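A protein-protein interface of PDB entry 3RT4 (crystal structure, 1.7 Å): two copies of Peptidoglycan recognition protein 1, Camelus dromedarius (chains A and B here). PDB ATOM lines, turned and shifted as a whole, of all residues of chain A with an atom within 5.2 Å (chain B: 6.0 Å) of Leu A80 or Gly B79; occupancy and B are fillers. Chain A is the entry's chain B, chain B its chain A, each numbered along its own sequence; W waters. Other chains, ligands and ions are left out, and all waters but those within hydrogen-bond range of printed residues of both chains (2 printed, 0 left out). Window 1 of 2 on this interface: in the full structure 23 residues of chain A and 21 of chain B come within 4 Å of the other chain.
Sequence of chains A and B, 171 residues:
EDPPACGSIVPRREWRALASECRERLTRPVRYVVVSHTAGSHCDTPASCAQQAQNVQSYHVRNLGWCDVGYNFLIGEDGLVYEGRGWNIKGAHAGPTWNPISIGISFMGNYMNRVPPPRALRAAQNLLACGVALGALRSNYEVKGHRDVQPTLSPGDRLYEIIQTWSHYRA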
ATOM      1  N   SER A   8     -20.759  18.990 -14.903  1.00  0.00           N
ATOM      2  CA  SER A   8     -19.746  20.064 -15.044  1.00  0.00           C
ATOM      3  C   SER A   8     -19.269  20.139 -16.484  1.00  0.00           C
ATOM      4  O   SER A   8     -18.069  20.122 -16.783  1.00  0.00           O
ATOM      5  CB  SER A   8     -18.541  19.789 -14.150  1.00  0.00           C
ATOM      6  OG  SER A   8     -18.954  19.320 -12.882  1.00  0.00           O
ATOM      7  N   VAL A  10     -18.515  21.746 -20.024  1.00  0.00           N
ATOM      8  CA  VAL A  10     -18.093  23.020 -20.563  1.00  0.00           C
ATOM      9  C   VAL A  10     -19.108  23.324 -21.679  1.00  0.00           C
ATOM     10  O   VAL A  10     -19.178  22.614 -22.681  1.00  0.00           O
ATOM     11  CB  VAL A  10     -16.683  22.960 -21.218  1.00  0.00           C
ATOM     12  CG1 VAL A  10     -16.373  24.307 -21.854  1.00  0.00           C
ATOM     13  CG2 VAL A  10     -15.615  22.594 -20.177  1.00  0.00           C
ATOM     14  N   PRO A  46      -7.759  23.197 -19.522  1.00  0.00           N
ATOM     15  CA  PRO A  46      -9.009  23.761 -20.042  1.00  0.00           C
ATOM     16  C   PRO A  46      -8.759  24.591 -21.319  1.00  0.00           C
ATOM     17  O   PRO A  46      -9.491  24.492 -22.305  1.00  0.00           O
ATOM     18  CB  PRO A  46      -9.478  24.629 -18.895  1.00  0.00           C
ATOM     19  CG  PRO A  46      -9.044  23.831 -17.675  1.00  0.00           C
ATOM     20  CD  PRO A  46      -7.664  23.337 -18.059  1.00  0.00           C
ATOM     21  N   LEU A  74     -17.587  15.573 -25.793  1.00  0.00           N
ATOM     22  CA  LEU A  74     -16.162  15.253 -25.938  1.00  0.00           C
ATOM     23  C   LEU A  74     -15.536  15.253 -24.534  1.00  0.00           C
ATOM     24  O   LEU A  74     -15.949  16.014 -23.657  1.00  0.00           O
ATOM     25  CB  LEU A  74     -15.418  16.273 -26.819  1.00  0.00           C
ATOM     26  CG  LEU A  74     -16.023  16.307 -28.231  1.00  0.00           C
ATOM     27  CD1 LEU A  74     -16.971  17.476 -28.325  1.00  0.00           C
ATOM     28  CD2 LEU A  74     -14.939  16.427 -29.301  1.00  0.00           C
ATOM     29  N   ILE A  75     -14.535  14.404 -24.334  1.00  0.00           N
ATOM     30  CA  ILE A  75     -13.838  14.300 -23.058  1.00  0.00           C
ATOM     31  C   ILE A  75     -12.378  14.666 -23.233  1.00  0.00           C
ATOM     32  O   ILE A  75     -11.665  14.111 -24.083  1.00  0.00           O
ATOM     33  CB  ILE A  75     -13.940  12.873 -22.497  1.00  0.00           C
ATOM     34  CG1 ILE A  75     -15.388  12.376 -22.682  1.00  0.00           C
ATOM     35  CG2 ILE A  75     -13.545  12.854 -21.021  1.00  0.00           C
ATOM     36  CD1 ILE A  75     -16.395  12.888 -21.652  1.00  0.00           C
ATOM     37  N   GLY A  76     -11.951  15.630 -22.437  1.00  0.00           N
ATOM     38  CA  GLY A  76     -10.578  16.054 -22.510  1.00  0.00           C
ATOM     39  C   GLY A  76      -9.709  15.454 -21.426  1.00  0.00           C
ATOM     40  O   GLY A  76     -10.195  14.980 -20.399  1.00  0.00           O
ATOM     41  N   ASP A  78      -7.971  17.066 -19.685  1.00  0.00           N
ATOM     42  CA  ASP A  78      -7.990  18.047 -18.602  1.00  0.00           C
ATOM     43  C   ASP A  78      -9.060  17.584 -17.573  1.00  0.00           C
ATOM     44  O   ASP A  78      -9.284  18.255 -16.566  1.00  0.00           O
ATOM     45  CB  ASP A  78      -8.396  19.442 -19.091  1.00  0.00           C
ATOM     46  CG  ASP A  78      -9.738  19.447 -19.827  1.00  0.00           C
ATOM     47  OD1 ASP A  78     -10.331  18.369 -20.048  1.00  0.00           O
ATOM     48  OD2 ASP A  78     -10.196  20.560 -20.192  1.00  0.00           O
ATOM     49  N   GLY A  79      -9.724  16.444 -17.805  1.00  0.00           N
ATOM     50  CA  GLY A  79     -10.736  15.989 -16.863  1.00  0.00           C
ATOM     51  C   GLY A  79     -12.082  16.690 -17.011  1.00  0.00           C
ATOM     52  O   GLY A  79     -12.914  16.626 -16.106  1.00  0.00           O
ATOM     53  N   LEU A  80     -12.302  17.394 -18.122  1.00  0.00           N
ATOM     54  CA  LEU A  80     -13.582  18.076 -18.325  1.00  0.00           C
ATOM     55  C   LEU A  80     -14.292  17.517 -19.539  1.00  0.00           C
ATOM     56  O   LEU A  80     -13.657  17.012 -20.464  1.00  0.00           O
ATOM     57  CB  LEU A  80     -13.398  19.581 -18.552  1.00  0.00           C
ATOM     58  CG  LEU A  80     -12.643  20.324 -17.452  1.00  0.00           C
ATOM     59  CD1 LEU A  80     -12.418  21.796 -17.813  1.00  0.00           C
ATOM     60  CD2 LEU A  80     -13.434  20.208 -16.167  1.00  0.00           C
ATOM     61  N   VAL A  81     -15.616  17.627 -19.519  1.00  0.00           N
ATOM     62  CA  VAL A  81     -16.467  17.192 -20.605  1.00  0.00           C
ATOM     63  C   VAL A  81     -16.851  18.468 -21.337  1.00  0.00           C
ATOM     64  O   VAL A  81     -17.161  19.477 -20.697  1.00  0.00           O
ATOM     65  CB  VAL A  81     -17.782  16.517 -20.096  1.00  0.00           C
ATOM     66  CG1 VAL A  81     -18.691  16.207 -21.292  1.00  0.00           C
ATOM     67  CG2 VAL A  81     -17.475  15.253 -19.281  1.00  0.00           C
ATOM     68  N   TYR A  82     -16.802  18.386 -22.672  1.00  0.00           N
ATOM     69  CA  TYR A  82     -17.131  19.451 -23.615  1.00  0.00           C
ATOM     70  C   TYR A  82     -18.457  19.140 -24.272  1.00  0.00           C
ATOM     71  O   TYR A  82     -18.668  18.046 -24.780  1.00  0.00           O
ATOM     72  CB  TYR A  82     -16.008  19.570 -24.624  1.00  0.00           C
ATOM     73  CG  TYR A  82     -14.825  20.174 -23.939  1.00  0.00           C
ATOM     74  CD1 TYR A  82     -13.975  19.403 -23.128  1.00  0.00           C
ATOM     75  CD2 TYR A  82     -14.638  21.544 -23.977  1.00  0.00           C
ATOM     76  CE1 TYR A  82     -12.970  20.005 -22.380  1.00  0.00           C
ATOM     77  CE2 TYR A  82     -13.655  22.153 -23.232  1.00  0.00           C
ATOM     78  CZ  TYR A  82     -12.814  21.382 -22.439  1.00  0.00           C
ATOM     79  OH  TYR A  82     -11.812  21.979 -21.717  1.00  0.00           O
ATOM     80  N   ALA A 123     -14.465  11.880 -15.665  1.00  0.00           N
ATOM     81  CA  ALA A 123     -15.354  12.856 -16.286  1.00  0.00           C
ATOM     82  C   ALA A 123     -16.407  12.136 -17.110  1.00  0.00           C
ATOM     83  O   ALA A 123     -17.571  12.525 -17.111  1.00  0.00           O
ATOM     84  CB  ALA A 123     -14.556  13.857 -17.161  1.00  0.00           C
ATOM     85  N   ILE B  75     -11.713  23.559  -4.661  1.00  0.00           N
ATOM     86  CA  ILE B  75     -12.115  23.739  -6.039  1.00  0.00           C
ATOM     87  C   ILE B  75     -11.018  24.468  -6.781  1.00  0.00           C
ATOM     88  O   ILE B  75     -10.581  25.528  -6.351  1.00  0.00           O
ATOM     89  CB  ILE B  75     -13.394  24.616  -6.174  1.00  0.00           C
ATOM     90  CG1 ILE B  75     -14.495  24.159  -5.215  1.00  0.00           C
ATOM     91  CG2 ILE B  75     -13.886  24.570  -7.615  1.00  0.00           C
ATOM     92  CD1 ILE B  75     -15.007  22.753  -5.439  1.00  0.00           C
ATOM     93  N   GLY B  76     -10.573  23.909  -7.894  1.00  0.00           N
ATOM     94  CA  GLY B  76      -9.555  24.589  -8.662  1.00  0.00           C
ATOM     95  C   GLY B  76     -10.095  25.317  -9.892  1.00  0.00           C
ATOM     96  O   GLY B  76     -11.183  24.989 -10.387  1.00  0.00           O
ATOM     97  N   GLU B  77      -9.364  26.333 -10.369  1.00  0.00           N
ATOM     98  CA  GLU B  77      -9.772  27.058 -11.565  1.00  0.00           C
ATOM     99  C   GLU B  77      -9.595  26.164 -12.806  1.00  0.00           C
ATOM    100  O   GLU B  77      -9.899  26.578 -13.934  1.00  0.00           O
ATOM    101  CB  GLU B  77      -8.995  28.362 -11.700  1.00  0.00           C
ATOM    102  CG  GLU B  77      -9.365  29.314 -10.598  1.00  0.00           C
ATOM    103  CD  GLU B  77      -8.973  30.750 -10.857  1.00  0.00           C
ATOM    104  OE1 GLU B  77      -8.610  31.100 -11.994  1.00  0.00           O
ATOM    105  OE2 GLU B  77      -9.040  31.540  -9.900  1.00  0.00           O
ATOM    106  N   ASP B  78      -9.079  24.953 -12.597  1.00  0.00           N
ATOM    107  CA  ASP B  78      -8.974  23.986 -13.683  1.00  0.00           C
ATOM    108  C   ASP B  78     -10.365  23.338 -13.853  1.00  0.00           C
ATOM    109  O   ASP B  78     -10.577  22.535 -14.767  1.00  0.00           O
ATOM    110  CB  ASP B  78      -7.945  22.876 -13.386  1.00  0.00           C
ATOM    111  CG  ASP B  78      -8.186  22.132 -12.052  1.00  0.00           C
ATOM    112  OD1 ASP B  78      -9.094  22.461 -11.248  1.00  0.00           O
ATOM    113  OD2 ASP B  78      -7.422  21.172 -11.833  1.00  0.00           O
ATOM    114  N   GLY B  79     -11.315  23.688 -12.981  1.00  0.00           N
ATOM    115  CA  GLY B  79     -12.655  23.121 -13.072  1.00  0.00           C
ATOM    116  C   GLY B  79     -12.832  21.777 -12.384  1.00  0.00           C
ATOM    117  O   GLY B  79     -13.862  21.119 -12.557  1.00  0.00           O
ATOM    118  N   LEU B  80     -11.831  21.370 -11.606  1.00  0.00           N
ATOM    119  CA  LEU B  80     -11.864  20.099 -10.895  1.00  0.00           C
ATOM    120  C   LEU B  80     -12.046  20.294  -9.407  1.00  0.00           C
ATOM    121  O   LEU B  80     -11.651  21.319  -8.854  1.00  0.00           O
ATOM    122  CB  LEU B  80     -10.565  19.336 -11.132  1.00  0.00           C
ATOM    123  CG  LEU B  80     -10.279  19.075 -12.615  1.00  0.00           C
ATOM    124  CD1 LEU B  80      -8.965  18.343 -12.714  1.00  0.00           C
ATOM    125  CD2 LEU B  80     -11.410  18.266 -13.282  1.00  0.00           C
ATOM    126  N   VAL B  81     -12.661  19.301  -8.784  1.00  0.00           N
ATOM    127  CA  VAL B  81     -12.885  19.272  -7.351  1.00  0.00           C
ATOM    128  C   VAL B  81     -11.803  18.352  -6.784  1.00  0.00           C
ATOM    129  O   VAL B  81     -11.589  17.253  -7.306  1.00  0.00           O
ATOM    130  CB  VAL B  81     -14.235  18.624  -6.987  1.00  0.00           C
ATOM    131  CG1 VAL B  81     -14.344  18.438  -5.466  1.00  0.00           C
ATOM    132  CG2 VAL B  81     -15.364  19.460  -7.544  1.00  0.00           C
ATOM    133  N   PRO B 117     -13.490  31.080 -12.594  1.00  0.00           N
ATOM    134  CA  PRO B 117     -14.093  30.939 -13.921  1.00  0.00           C
ATOM    135  C   PRO B 117     -15.340  30.090 -13.758  1.00  0.00           C
ATOM    136  O   PRO B 117     -15.449  29.355 -12.788  1.00  0.00           O
ATOM    137  CB  PRO B 117     -13.033  30.183 -14.690  1.00  0.00           C
ATOM    138  CG  PRO B 117     -12.357  29.341 -13.593  1.00  0.00           C
ATOM    139  CD  PRO B 117     -12.187  30.399 -12.546  1.00  0.00           C
ATOM    140  N   ARG B 119     -16.102  27.370 -14.991  1.00  0.00           N
ATOM    141  CA  ARG B 119     -15.882  25.939 -14.739  1.00  0.00           C
ATOM    142  C   ARG B 119     -15.691  25.581 -13.262  1.00  0.00           C
ATOM    143  O   ARG B 119     -16.082  24.494 -12.828  1.00  0.00           O
ATOM    144  CB  ARG B 119     -14.716  25.378 -15.561  1.00  0.00           C
ATOM    145  CG  ARG B 119     -13.347  25.859 -15.208  1.00  0.00           C
ATOM    146  CD  ARG B 119     -12.343  25.367 -16.222  1.00  0.00           C
ATOM    147  NE  ARG B 119     -11.235  26.285 -16.116  1.00  0.00           N
ATOM    148  CZ  ARG B 119     -11.022  27.320 -16.912  1.00  0.00           C
ATOM    149  NH1 ARG B 119     -11.795  27.587 -17.968  1.00  0.00           N
ATOM    150  NH2 ARG B 119     -10.097  28.177 -16.535  1.00  0.00           N
ATOM    151  N   ALA B 120     -15.102  26.495 -12.496  1.00  0.00           N
ATOM    152  CA  ALA B 120     -14.886  26.255 -11.082  1.00  0.00           C
ATOM    153  C   ALA B 120     -16.229  26.329 -10.368  1.00  0.00           C
ATOM    154  O   ALA B 120     -16.521  25.535  -9.472  1.00  0.00           O
ATOM    155  CB  ALA B 120     -13.926  27.294 -10.515  1.00  0.00           C
ATOM    156  N   ARG B 122     -19.186  25.739 -11.693  1.00  0.00           N
ATOM    157  CA  ARG B 122     -19.966  24.550 -12.027  1.00  0.00           C
ATOM    158  C   ARG B 122     -19.534  23.351 -11.219  1.00  0.00           C
ATOM    159  O   ARG B 122     -20.378  22.584 -10.778  1.00  0.00           O
ATOM    160  CB  ARG B 122     -19.811  24.143 -13.482  1.00  0.00           C
ATOM    161  CG  ARG B 122     -20.664  24.914 -14.421  1.00  0.00           C
ATOM    162  CD  ARG B 122     -20.514  24.387 -15.827  1.00  0.00           C
ATOM    163  NE  ARG B 122     -19.149  24.282 -16.354  1.00  0.00           N
ATOM    164  CZ  ARG B 122     -18.576  25.209 -17.114  1.00  0.00           C
ATOM    165  NH1 ARG B 122     -17.339  25.057 -17.560  1.00  0.00           N
ATOM    166  NH2 ARG B 122     -19.227  26.333 -17.371  1.00  0.00           N
ATOM    167  N   ALA B 123     -18.231  23.174 -11.023  1.00  0.00           N
ATOM    168  CA  ALA B 123     -17.733  22.016 -10.291  1.00  0.00           C
ATOM    169  C   ALA B 123     -18.239  22.046  -8.864  1.00  0.00           C
ATOM    170  O   ALA B 123     -18.687  21.030  -8.321  1.00  0.00           O
ATOM    171  CB  ALA B 123     -16.206  21.999 -10.319  1.00  0.00           C
HETATM  172  O   HOH W   1     -16.642  22.524 -16.821  1.00  0.00           O
HETATM  173  O   HOH W   2      -8.708  20.903 -16.053  1.00  0.00           O
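Of the printed residues of chain B, Val A10 touches Arg B122 (3.7 Å).
Of the printed residues of chain B, Gly A79 touches Leu B80 (3.6 Å).
Of chain B, only Asp B78, Gly B79 and Arg B119 come within 4 Å of Leu A80.
Ala A123 touches none of the printed residues of chain B.
Gly B76 touches none of the printed residues of chain A.
Of chain A, only Leu A80 (3.7 Å) comes within 4 Å of Gly B79.
Of the printed residues of chain A, Ala B123 touches Ser A8 (3.9 Å).
The nearest residue of chain B that does not touch Leu A80 is Leu B80 (4.02 Å).
Asp A78 touches Leu B80, and with the chains exchanged Leu A80 touches Asp B78.
Gly A79 touches Leu B80, and with the chains exchanged Leu A80 touches Gly B79.
Hydrophobic or aromatic side chains of chain A within 4 Å of the printed part of chain B: Val A10, Pro A46 and Leu A80.
Of the 12 printed residues of chain B, 6 touch a printed residue of chain A.
Among the printed residues, no Asp or Glu carboxylate lies within 4 Å of a Lys or Arg side-chain nitrogen of the other chain.
Water W1 bridges NH1 of Arg B122 and O of Ser A8.
Water W2 bridges O of Asp A78 (2.8 Å) and O of Asp B78 (2.8 Å).
The backbone carbonyl oxygen (O) of Glu B77 lies within hydrogen-bond range of the guanidinium group (NE) of Arg B119 (2.6 Å).
The backbone NH (N) of Leu A80 sits at hydrogen-bond distance from the side-chain carboxylate (OD1) of Asp A78 (2.9 Å).
OD1 of Asp B78 sits at hydrogen-bond distance from N of Leu B80.
OD2 of Asp A78 sits at hydrogen-bond distance from OH of Tyr A82 (2.6 Å).
The backbone carbonyl oxygen (O) of Val A81 is in hydrogen-bond range of the backbone NH (N) of Val A10 (2.7 Å).
The backbone carbonyl oxygen (O) of Pro A46 sits at hydrogen-bond distance from the side-chain hydroxyl (OH) of Tyr A82, 3.5 Å away.
Among the printed residues, pairs that only touch across the chains: Pro A46 with Asp B78 (3.5 Å), Gly A79 with Leu B80 (3.6 Å), Leu A80 with Asp B78 (3.6 Å), Pro A46 with Arg B119 (3.6 Å), Val A10 with Arg B122 (3.7 Å), Leu A80 with Gly B79 (3.7 Å), Asp A78 with Leu B80 (3.9 Å), Leu A80 with Arg B119 (3.9 Å) and Ser A8 with Ala B123 (3.9 Å).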
